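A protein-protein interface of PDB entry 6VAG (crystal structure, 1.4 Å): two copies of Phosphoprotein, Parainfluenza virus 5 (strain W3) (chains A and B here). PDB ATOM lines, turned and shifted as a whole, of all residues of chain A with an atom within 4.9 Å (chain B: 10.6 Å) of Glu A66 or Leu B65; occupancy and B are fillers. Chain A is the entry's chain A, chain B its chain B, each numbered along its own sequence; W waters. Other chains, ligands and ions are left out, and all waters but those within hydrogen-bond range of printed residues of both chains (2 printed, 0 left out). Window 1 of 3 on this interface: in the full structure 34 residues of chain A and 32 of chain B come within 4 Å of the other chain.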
ATOM      1  N   MET A  62     -11.295 -27.211   4.678  1.00  0.00           N
ATOM      2  CA  MET A  62     -12.694 -26.868   4.917  1.00  0.00           C
ATOM      3  C   MET A  62     -13.564 -28.112   4.978  1.00  0.00           C
ATOM      4  O   MET A  62     -14.536 -28.159   5.746  1.00  0.00           O
ATOM      5  CB  MET A  62     -13.194 -25.894   3.850  1.00  0.00           C
ATOM      6  CG  MET A  62     -12.580 -24.500   3.977  1.00  0.00           C
ATOM      7  SD  MET A  62     -13.145 -23.362   2.699  1.00  0.00           S
ATOM      8  CE  MET A  62     -14.901 -23.354   3.036  1.00  0.00           C
ATOM      9  N   ASN A  63     -13.225 -29.132   4.194  1.00  0.00           N
ATOM     10  CA  ASN A  63     -13.920 -30.405   4.295  1.00  0.00           C
ATOM     11  C   ASN A  63     -13.757 -31.005   5.689  1.00  0.00           C
ATOM     12  O   ASN A  63     -14.735 -31.441   6.306  1.00  0.00           O
ATOM     13  CB  ASN A  63     -13.408 -31.355   3.216  1.00  0.00           C
ATOM     14  CG  ASN A  63     -14.160 -32.660   3.205  1.00  0.00           C
ATOM     15  OD1 ASN A  63     -15.317 -32.714   2.788  1.00  0.00           O
ATOM     16  ND2 ASN A  63     -13.518 -33.718   3.682  1.00  0.00           N
ATOM     17  N   GLN A  64     -12.522 -31.031   6.203  1.00  0.00           N
ATOM     18  CA  GLN A  64     -12.289 -31.545   7.550  1.00  0.00           C
ATOM     19  C   GLN A  64     -13.002 -30.690   8.589  1.00  0.00           C
ATOM     20  O   GLN A  64     -13.561 -31.214   9.563  1.00  0.00           O
ATOM     21  CB  GLN A  64     -10.789 -31.574   7.851  1.00  0.00           C
ATOM     22  CG  GLN A  64      -9.953 -32.373   6.874  1.00  0.00           C
ATOM     23  CD  GLN A  64      -8.475 -31.998   6.933  1.00  0.00           C
ATOM     24  OE1 GLN A  64      -7.725 -32.237   5.986  1.00  0.00           O
ATOM     25  NE2 GLN A  64      -8.053 -31.414   8.054  1.00  0.00           N
ATOM     26  N   LEU A  65     -12.988 -29.369   8.405  1.00  0.00           N
ATOM     27  CA  LEU A  65     -13.664 -28.486   9.348  1.00  0.00           C
ATOM     28  C   LEU A  65     -15.151 -28.797   9.408  1.00  0.00           C
ATOM     29  O   LEU A  65     -15.744 -28.835  10.494  1.00  0.00           O
ATOM     30  CB  LEU A  65     -13.435 -27.024   8.950  1.00  0.00           C
ATOM     31  CG  LEU A  65     -13.674 -25.976  10.043  1.00  0.00           C
ATOM     32  CD1 LEU A  65     -12.658 -26.131  11.157  1.00  0.00           C
ATOM     33  CD2 LEU A  65     -13.643 -24.564   9.466  1.00  0.00           C
ATOM     34  N   GLU A  66     -15.772 -29.030   8.251  1.00  0.00           N
ATOM     35  CA  GLU A  66     -17.196 -29.334   8.230  1.00  0.00           C
ATOM     36  C   GLU A  66     -17.493 -30.623   8.981  1.00  0.00           C
ATOM     37  O   GLU A  66     -18.520 -30.728   9.664  1.00  0.00           O
ATOM     38  CB  GLU A  66     -17.702 -29.423   6.790  1.00  0.00           C
ATOM     39  CG  GLU A  66     -19.199 -29.689   6.726  1.00  0.00           C
ATOM     40  CD  GLU A  66     -19.812 -29.391   5.379  1.00  0.00           C
ATOM     41  OE1 GLU A  66     -19.064 -29.018   4.456  1.00  0.00           O
ATOM     42  OE2 GLU A  66     -21.049 -29.527   5.253  1.00  0.00           O
ATOM     43  N   THR A  67     -16.612 -31.620   8.861  1.00  0.00           N
ATOM     44  CA  THR A  67     -16.808 -32.862   9.599  1.00  0.00           C
ATOM     45  C   THR A  67     -16.820 -32.602  11.097  1.00  0.00           C
ATOM     46  O   THR A  67     -17.650 -33.156  11.826  1.00  0.00           O
ATOM     47  CB  THR A  67     -15.710 -33.862   9.244  1.00  0.00           C
ATOM     48  OG1 THR A  67     -15.814 -34.211   7.857  1.00  0.00           O
ATOM     49  CG2 THR A  67     -15.843 -35.126  10.092  1.00  0.00           C
ATOM     50  N   LYS A  68     -15.907 -31.757  11.579  1.00  0.00           N
ATOM     51  CA  LYS A  68     -15.875 -31.456  13.005  1.00  0.00           C
ATOM     52  C   LYS A  68     -17.087 -30.632  13.416  1.00  0.00           C
ATOM     53  O   LYS A  68     -17.623 -30.819  14.514  1.00  0.00           O
ATOM     54  CB  LYS A  68     -14.569 -30.749  13.369  1.00  0.00           C
ATOM     55  CG  LYS A  68     -13.345 -31.652  13.272  1.00  0.00           C
ATOM     56  CD  LYS A  68     -12.080 -30.951  13.732  1.00  0.00           C
ATOM     57  CE  LYS A  68     -10.935 -31.940  13.908  1.00  0.00           C
ATOM     58  NZ  LYS A  68      -9.610 -31.273  13.788  1.00  0.00           N
ATOM     59  N   VAL A  69     -17.536 -29.719  12.553  1.00  0.00           N
ATOM     60  CA  VAL A  69     -18.751 -28.957  12.826  1.00  0.00           C
ATOM     61  C   VAL A  69     -19.950 -29.896  12.916  1.00  0.00           C
ATOM     62  O   VAL A  69     -20.848 -29.709  13.748  1.00  0.00           O
ATOM     63  CB  VAL A  69     -18.927 -27.857  11.758  1.00  0.00           C
ATOM     64  CG1 VAL A  69     -20.336 -27.287  11.769  1.00  0.00           C
ATOM     65  CG2 VAL A  69     -17.903 -26.753  11.981  1.00  0.00           C
ATOM     66  N   ASP A  70     -19.972 -30.931  12.071  1.00  0.00           N
ATOM     67  CA  ASP A  70     -21.012 -31.954  12.151  1.00  0.00           C
ATOM     68  C   ASP A  70     -21.013 -32.623  13.519  1.00  0.00           C
ATOM     69  O   ASP A  70     -22.074 -32.843  14.119  1.00  0.00           O
ATOM     70  CB  ASP A  70     -20.785 -33.011  11.066  1.00  0.00           C
ATOM     71  CG  ASP A  70     -21.208 -32.551   9.684  1.00  0.00           C
ATOM     72  OD1 ASP A  70     -22.015 -31.603   9.583  1.00  0.00           O
ATOM     73  OD2 ASP A  70     -20.737 -33.151   8.692  1.00  0.00           O
ATOM     74  N   ASN B  57     -15.728 -24.170  -5.521  1.00  0.00           N
ATOM     75  CA  ASN B  57     -16.028 -25.200  -4.531  1.00  0.00           C
ATOM     76  C   ASN B  57     -15.869 -24.674  -3.105  1.00  0.00           C
ATOM     77  O   ASN B  57     -16.662 -25.025  -2.224  1.00  0.00           O
ATOM     78  CB  ASN B  57     -15.147 -26.426  -4.773  1.00  0.00           C
ATOM     79  CG  ASN B  57     -15.583 -27.230  -5.984  1.00  0.00           C
ATOM     80  OD1 ASN B  57     -16.702 -27.078  -6.481  1.00  0.00           O
ATOM     81  ND2 ASN B  57     -14.696 -28.093  -6.468  1.00  0.00           N
ATOM     82  N   LEU B  58     -14.853 -23.838  -2.849  1.00  0.00           N
ATOM     83  CA  LEU B  58     -14.712 -23.240  -1.519  1.00  0.00           C
ATOM     84  C   LEU B  58     -15.929 -22.389  -1.172  1.00  0.00           C
ATOM     85  O   LEU B  58     -16.388 -22.386  -0.025  1.00  0.00           O
ATOM     86  CB  LEU B  58     -13.450 -22.377  -1.428  1.00  0.00           C
ATOM     87  CG  LEU B  58     -12.070 -23.001  -1.637  1.00  0.00           C
ATOM     88  CD1 LEU B  58     -11.002 -21.951  -1.360  1.00  0.00           C
ATOM     89  CD2 LEU B  58     -11.866 -24.217  -0.765  1.00  0.00           C
ATOM     90  N   ASP B  59     -16.445 -21.639  -2.147  1.00  0.00           N
ATOM     91  CA  ASP B  59     -17.641 -20.828  -1.942  1.00  0.00           C
ATOM     92  C   ASP B  59     -18.818 -21.703  -1.514  1.00  0.00           C
ATOM     93  O   ASP B  59     -19.537 -21.379  -0.556  1.00  0.00           O
ATOM     94  CB  ASP B  59     -17.921 -20.072  -3.249  1.00  0.00           C
ATOM     95  CG  ASP B  59     -18.930 -18.939  -3.105  1.00  0.00           C
ATOM     96  OD1 ASP B  59     -19.530 -18.770  -2.021  1.00  0.00           O
ATOM     97  OD2 ASP B  59     -19.117 -18.211  -4.113  1.00  0.00           O
ATOM     98  N   SER B  60     -19.004 -22.838  -2.190  1.00  0.00           N
ATOM     99  CA  SER B  60     -20.088 -23.750  -1.837  1.00  0.00           C
ATOM    100  C   SER B  60     -19.873 -24.344  -0.454  1.00  0.00           C
ATOM    101  O   SER B  60     -20.814 -24.443   0.346  1.00  0.00           O
ATOM    102  CB  SER B  60     -20.151 -24.878  -2.859  1.00  0.00           C
ATOM    103  OG  SER B  60     -20.454 -24.377  -4.144  1.00  0.00           O
ATOM    104  N   ARG B  61     -18.639 -24.752  -0.155  1.00  0.00           N
ATOM    105  CA  ARG B  61     -18.345 -25.296   1.166  1.00  0.00           C
ATOM    106  C   ARG B  61     -18.625 -24.268   2.253  1.00  0.00           C
ATOM    107  O   ARG B  61     -19.141 -24.609   3.326  1.00  0.00           O
ATOM    108  CB  ARG B  61     -16.881 -25.730   1.230  1.00  0.00           C
ATOM    109  CG  ARG B  61     -16.576 -27.041   0.524  1.00  0.00           C
ATOM    110  CD  ARG B  61     -15.155 -27.508   0.816  1.00  0.00           C
ATOM    111  NE  ARG B  61     -14.838 -28.730   0.084  1.00  0.00           N
ATOM    112  CZ  ARG B  61     -15.304 -29.932   0.406  1.00  0.00           C
ATOM    113  NH1 ARG B  61     -16.099 -30.082   1.458  1.00  0.00           N
ATOM    114  NH2 ARG B  61     -14.966 -30.990  -0.321  1.00  0.00           N
ATOM    115  N   MET B  62     -18.276 -23.007   1.998  1.00  0.00           N
ATOM    116  CA  MET B  62     -18.487 -21.957   2.985  1.00  0.00           C
ATOM    117  C   MET B  62     -19.972 -21.754   3.268  1.00  0.00           C
ATOM    118  O   MET B  62     -20.358 -21.490   4.412  1.00  0.00           O
ATOM    119  CB  MET B  62     -17.831 -20.662   2.507  1.00  0.00           C
ATOM    120  CG  MET B  62     -17.829 -19.555   3.551  1.00  0.00           C
ATOM    121  SD  MET B  62     -16.928 -19.960   5.070  1.00  0.00           S
ATOM    122  CE  MET B  62     -15.424 -20.688   4.449  1.00  0.00           C
ATOM    123  N   ASN B  63     -20.822 -21.874   2.244  1.00  0.00           N
ATOM    124  CA  ASN B  63     -22.265 -21.827   2.470  1.00  0.00           C
ATOM    125  C   ASN B  63     -22.685 -22.901   3.460  1.00  0.00           C
ATOM    126  O   ASN B  63     -23.493 -22.653   4.366  1.00  0.00           O
ATOM    127  CB  ASN B  63     -23.019 -22.046   1.154  1.00  0.00           C
ATOM    128  CG  ASN B  63     -22.811 -20.932   0.152  1.00  0.00           C
ATOM    129  OD1 ASN B  63     -22.480 -19.803   0.512  1.00  0.00           O
ATOM    130  ND2 ASN B  63     -23.026 -21.245  -1.127  1.00  0.00           N
ATOM    131  N   GLN B  64     -22.147 -24.111   3.297  1.00  0.00           N
ATOM    132  CA  GLN B  64     -22.504 -25.210   4.192  1.00  0.00           C
ATOM    133  C   GLN B  64     -22.021 -24.938   5.611  1.00  0.00           C
ATOM    134  O   GLN B  64     -22.759 -25.141   6.583  1.00  0.00           O
ATOM    135  CB  GLN B  64     -21.918 -26.523   3.665  1.00  0.00           C
ATOM    136  CG  GLN B  64     -22.555 -27.029   2.378  1.00  0.00           C
ATOM    137  CD  GLN B  64     -21.599 -27.861   1.539  1.00  0.00           C
ATOM    138  OE1 GLN B  64     -20.608 -28.394   2.045  1.00  0.00           O
ATOM    139  NE2 GLN B  64     -21.899 -27.988   0.253  1.00  0.00           N
ATOM    140  N   LEU B  65     -20.778 -24.480   5.751  1.00  0.00           N
ATOM    141  CA  LEU B  65     -20.233 -24.178   7.070  1.00  0.00           C
ATOM    142  C   LEU B  65     -21.045 -23.091   7.759  1.00  0.00           C
ATOM    143  O   LEU B  65     -21.373 -23.204   8.947  1.00  0.00           O
ATOM    144  CB  LEU B  65     -18.771 -23.751   6.938  1.00  0.00           C
ATOM    145  CG  LEU B  65     -17.737 -24.858   6.768  1.00  0.00           C
ATOM    146  CD1 LEU B  65     -16.373 -24.261   6.419  1.00  0.00           C
ATOM    147  CD2 LEU B  65     -17.650 -25.714   8.024  1.00  0.00           C
ATOM    148  N   GLU B  66     -21.384 -22.031   7.029  1.00  0.00           N
ATOM    149  CA  GLU B  66     -22.135 -20.934   7.627  1.00  0.00           C
ATOM    150  C   GLU B  66     -23.483 -21.413   8.149  1.00  0.00           C
ATOM    151  O   GLU B  66     -23.895 -21.050   9.257  1.00  0.00           O
ATOM    152  CB  GLU B  66     -22.317 -19.808   6.614  1.00  0.00           C
ATOM    153  CG  GLU B  66     -21.027 -19.098   6.232  1.00  0.00           C
ATOM    154  CD  GLU B  66     -21.194 -18.174   5.040  1.00  0.00           C
ATOM    155  OE1 GLU B  66     -22.069 -18.437   4.181  1.00  0.00           O
ATOM    156  OE2 GLU B  66     -20.455 -17.172   4.971  1.00  0.00           O
ATOM    157  N   THR B  67     -24.190 -22.221   7.357  1.00  0.00           N
ATOM    158  CA  THR B  67     -25.490 -22.723   7.778  1.00  0.00           C
ATOM    159  C   THR B  67     -25.366 -23.566   9.041  1.00  0.00           C
ATOM    160  O   THR B  67     -26.199 -23.464   9.956  1.00  0.00           O
ATOM    161  CB  THR B  67     -26.098 -23.547   6.645  1.00  0.00           C
ATOM    162  OG1 THR B  67     -26.427 -22.679   5.557  1.00  0.00           O
ATOM    163  CG2 THR B  67     -27.351 -24.269   7.126  1.00  0.00           C
ATOM    164  N   LYS B  68     -24.335 -24.406   9.113  1.00  0.00           N
ATOM    165  CA  LYS B  68     -24.206 -25.306  10.254  1.00  0.00           C
ATOM    166  C   LYS B  68     -23.741 -24.568  11.503  1.00  0.00           C
ATOM    167  O   LYS B  68     -24.196 -24.871  12.612  1.00  0.00           O
ATOM    168  CB  LYS B  68     -23.289 -26.476   9.901  1.00  0.00           C
ATOM    169  CG  LYS B  68     -23.889 -27.405   8.853  1.00  0.00           C
ATOM    170  CD  LYS B  68     -22.956 -28.554   8.515  1.00  0.00           C
ATOM    171  CE  LYS B  68     -23.626 -29.533   7.557  1.00  0.00           C
ATOM    172  NZ  LYS B  68     -22.766 -30.709   7.245  1.00  0.00           N
ATOM    173  N   VAL B  69     -22.861 -23.580  11.351  1.00  0.00           N
ATOM    174  CA  VAL B  69     -22.453 -22.783  12.501  1.00  0.00           C
ATOM    175  C   VAL B  69     -23.627 -21.977  13.041  1.00  0.00           C
ATOM    176  O   VAL B  69     -23.801 -21.852  14.261  1.00  0.00           O
ATOM    177  CB  VAL B  69     -21.235 -21.909  12.146  1.00  0.00           C
ATOM    178  CG1 VAL B  69     -21.002 -20.865  13.226  1.00  0.00           C
ATOM    179  CG2 VAL B  69     -19.999 -22.787  11.968  1.00  0.00           C
ATOM    180  N   ASP B  70     -24.467 -21.436  12.154  1.00  0.00           N
ATOM    181  CA  ASP B  70     -25.676 -20.754  12.611  1.00  0.00           C
ATOM    182  C   ASP B  70     -26.574 -21.705  13.394  1.00  0.00           C
ATOM    183  O   ASP B  70     -27.194 -21.312  14.394  1.00  0.00           O
ATOM    184  CB  ASP B  70     -26.433 -20.172  11.417  1.00  0.00           C
ATOM    185  CG  ASP B  70     -25.818 -18.877  10.905  1.00  0.00           C
ATOM    186  OD1 ASP B  70     -24.932 -18.322  11.589  1.00  0.00           O
ATOM    187  OD2 ASP B  70     -26.210 -18.419   9.808  1.00  0.00           O
ATOM    188  N   ARG B  71     -26.658 -22.962  12.958  1.00  0.00           N
ATOM    189  CA  ARG B  71     -27.439 -23.948  13.697  1.00  0.00           C
ATOM    190  C   ARG B  71     -26.880 -24.141  15.101  1.00  0.00           C
ATOM    191  O   ARG B  71     -27.628 -24.138  16.086  1.00  0.00           O
ATOM    192  CB  ARG B  71     -27.459 -25.275  12.938  1.00  0.00           C
ATOM    193  CG  ARG B  71     -28.615 -25.414  11.967  1.00  0.00           C
ATOM    194  CD  ARG B  71     -29.236 -26.809  12.048  1.00  0.00           C
ATOM    195  NE  ARG B  71     -28.347 -27.838  11.512  1.00  0.00           N
ATOM    196  CZ  ARG B  71     -28.038 -27.960  10.225  1.00  0.00           C
ATOM    197  NH1 ARG B  71     -28.543 -27.113   9.338  1.00  0.00           N
ATOM    198  NH2 ARG B  71     -27.222 -28.926   9.823  1.00  0.00           N
ATOM    199  N   ILE B  72     -25.565 -24.322  15.213  1.00  0.00           N
ATOM    200  CA  ILE B  72     -24.945 -24.484  16.526  1.00  0.00           C
ATOM    201  C   ILE B  72     -25.233 -23.273  17.402  1.00  0.00           C
ATOM    202  O   ILE B  72     -25.637 -23.404  18.564  1.00  0.00           O
ATOM    203  CB  ILE B  72     -23.436 -24.740  16.380  1.00  0.00           C
ATOM    204  CG1 ILE B  72     -23.197 -26.054  15.636  1.00  0.00           C
ATOM    205  CG2 ILE B  72     -22.762 -24.753  17.751  1.00  0.00           C
ATOM    206  CD1 ILE B  72     -21.779 -26.223  15.139  1.00  0.00           C
ATOM    207  N   LEU B  73     -25.047 -22.075  16.849  1.00  0.00           N
ATOM    208  CA  LEU B  73     -25.187 -20.856  17.634  1.00  0.00           C
ATOM    209  C   LEU B  73     -26.600 -20.712  18.185  1.00  0.00           C
ATOM    210  O   LEU B  73     -26.790 -20.265  19.325  1.00  0.00           O
ATOM    211  CB  LEU B  73     -24.802 -19.651  16.776  1.00  0.00           C
ATOM    212  CG  LEU B  73     -24.587 -18.323  17.496  1.00  0.00           C
ATOM    213  CD1 LEU B  73     -23.449 -18.437  18.501  1.00  0.00           C
ATOM    214  CD2 LEU B  73     -24.306 -17.223  16.485  1.00  0.00           C
HETATM  215  O   HOH W   1     -22.750 -29.968   3.359  1.00  0.00           O
HETATM  216  O   HOH W   2     -16.818 -28.397   3.666  1.00  0.00           O
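Met A62 touches its own counterpart, Met B62. Met A62 touches Leu B65, but with the chains exchanged Leu A65 does not touch Met B62 (6.6 Å). Glu A66 touches Leu B65, but with the chains exchanged Leu A65 does not touch Glu B66 (8.5 Å). Asp A70 touches Lys B68, but with the chains exchanged Lys A68 does not touch Asp B70 (11.9 Å). Positions printed for both chains: 62, 63, 64, 65, 66, 67, 68, 69 and 70.
OD1 of Asn A63 lies within hydrogen-bond range of NH1 of Arg B61, 3.1 Å away. The side-chain carboxylate of Glu A66 lies close to the side-chain amide oxygen of Gln B64 (2.9 Å). The side-chain carboxylate of Glu A66 is in salt-bridge range of the side-chain amino group of Lys B68. OD1 of Asp A70 lies within salt-bridge range of NZ of Lys B68 (2.6 Å).
Printed residues of chain A that touch a printed residue of chain B: Met A62, Asn A63, Glu A66, Val A69 and Asp A70. Hydrophobic or aromatic side chains of chain A within 4 Å of the printed part of chain B: Met A62 and Val A69. Of the 17 printed residues of chain B, 7 touch a printed residue of chain A. Hydrophobic or aromatic side chains of chain B within 4 Å of the printed part of chain A: Leu B58, Met B62, Leu B65 and Ile B72.
Among the printed residues, pairs that only touch across the chains: Met A62 with Met B62 (3.1 Å), Met A62 with Leu B58 (3.5 Å), Met A62 with Arg B61 (3.6 Å), Val A69 with Lys B68 (3.6 Å), Glu A66 with Leu B65 (3.7 Å), Met A62 with Leu B65 (3.8 Å) and Val A69 with Ile B72 (3.8 Å).
Water W2 lies within hydrogen-bond range of the side-chain carboxylate of Glu A66, the guanidinium group of Arg B61 and the backbone carbonyl oxygen of Met A62. Water W1 lies within hydrogen-bond range of OE2 of Glu A66 (2.6 Å) and OE1 of Gln B64 (3.0 Å).
Of chain B, only Gln B64 (2.9 Å), Leu B65 (3.7 Å) and Lys B68 (2.9 Å) come within 4 Å of Glu A66. Of chain A, only Met A62 (3.8 Å) and Glu A66 (3.7 Å) come within 4 Å of Leu B65. No residue of chain B comes within 4 Å of Thr A67. Of the printed residues of chain A, Met B62 touches Met A62 (3.1 Å). Of the printed residues of chain A, Gln B64 touches Glu A66. Printed residues of chain A within 4 Å of Arg B61: Met A62 (3.6 Å) and Asn A63 (3.1 Å). Val B69 touches none of the printed residues of chain A. Leu B73 touches none of the printed residues of chain A. The nearest residue of chain B that does not touch Glu A66 is Arg B61 (4.3 Å). The nearest printed residue of chain A that does not touch Lys B68 is Thr A67 (6.4 Å).
O of Asn A63 sits at hydrogen-bond distance from OG1 of Thr A67, 3.4 Å away.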
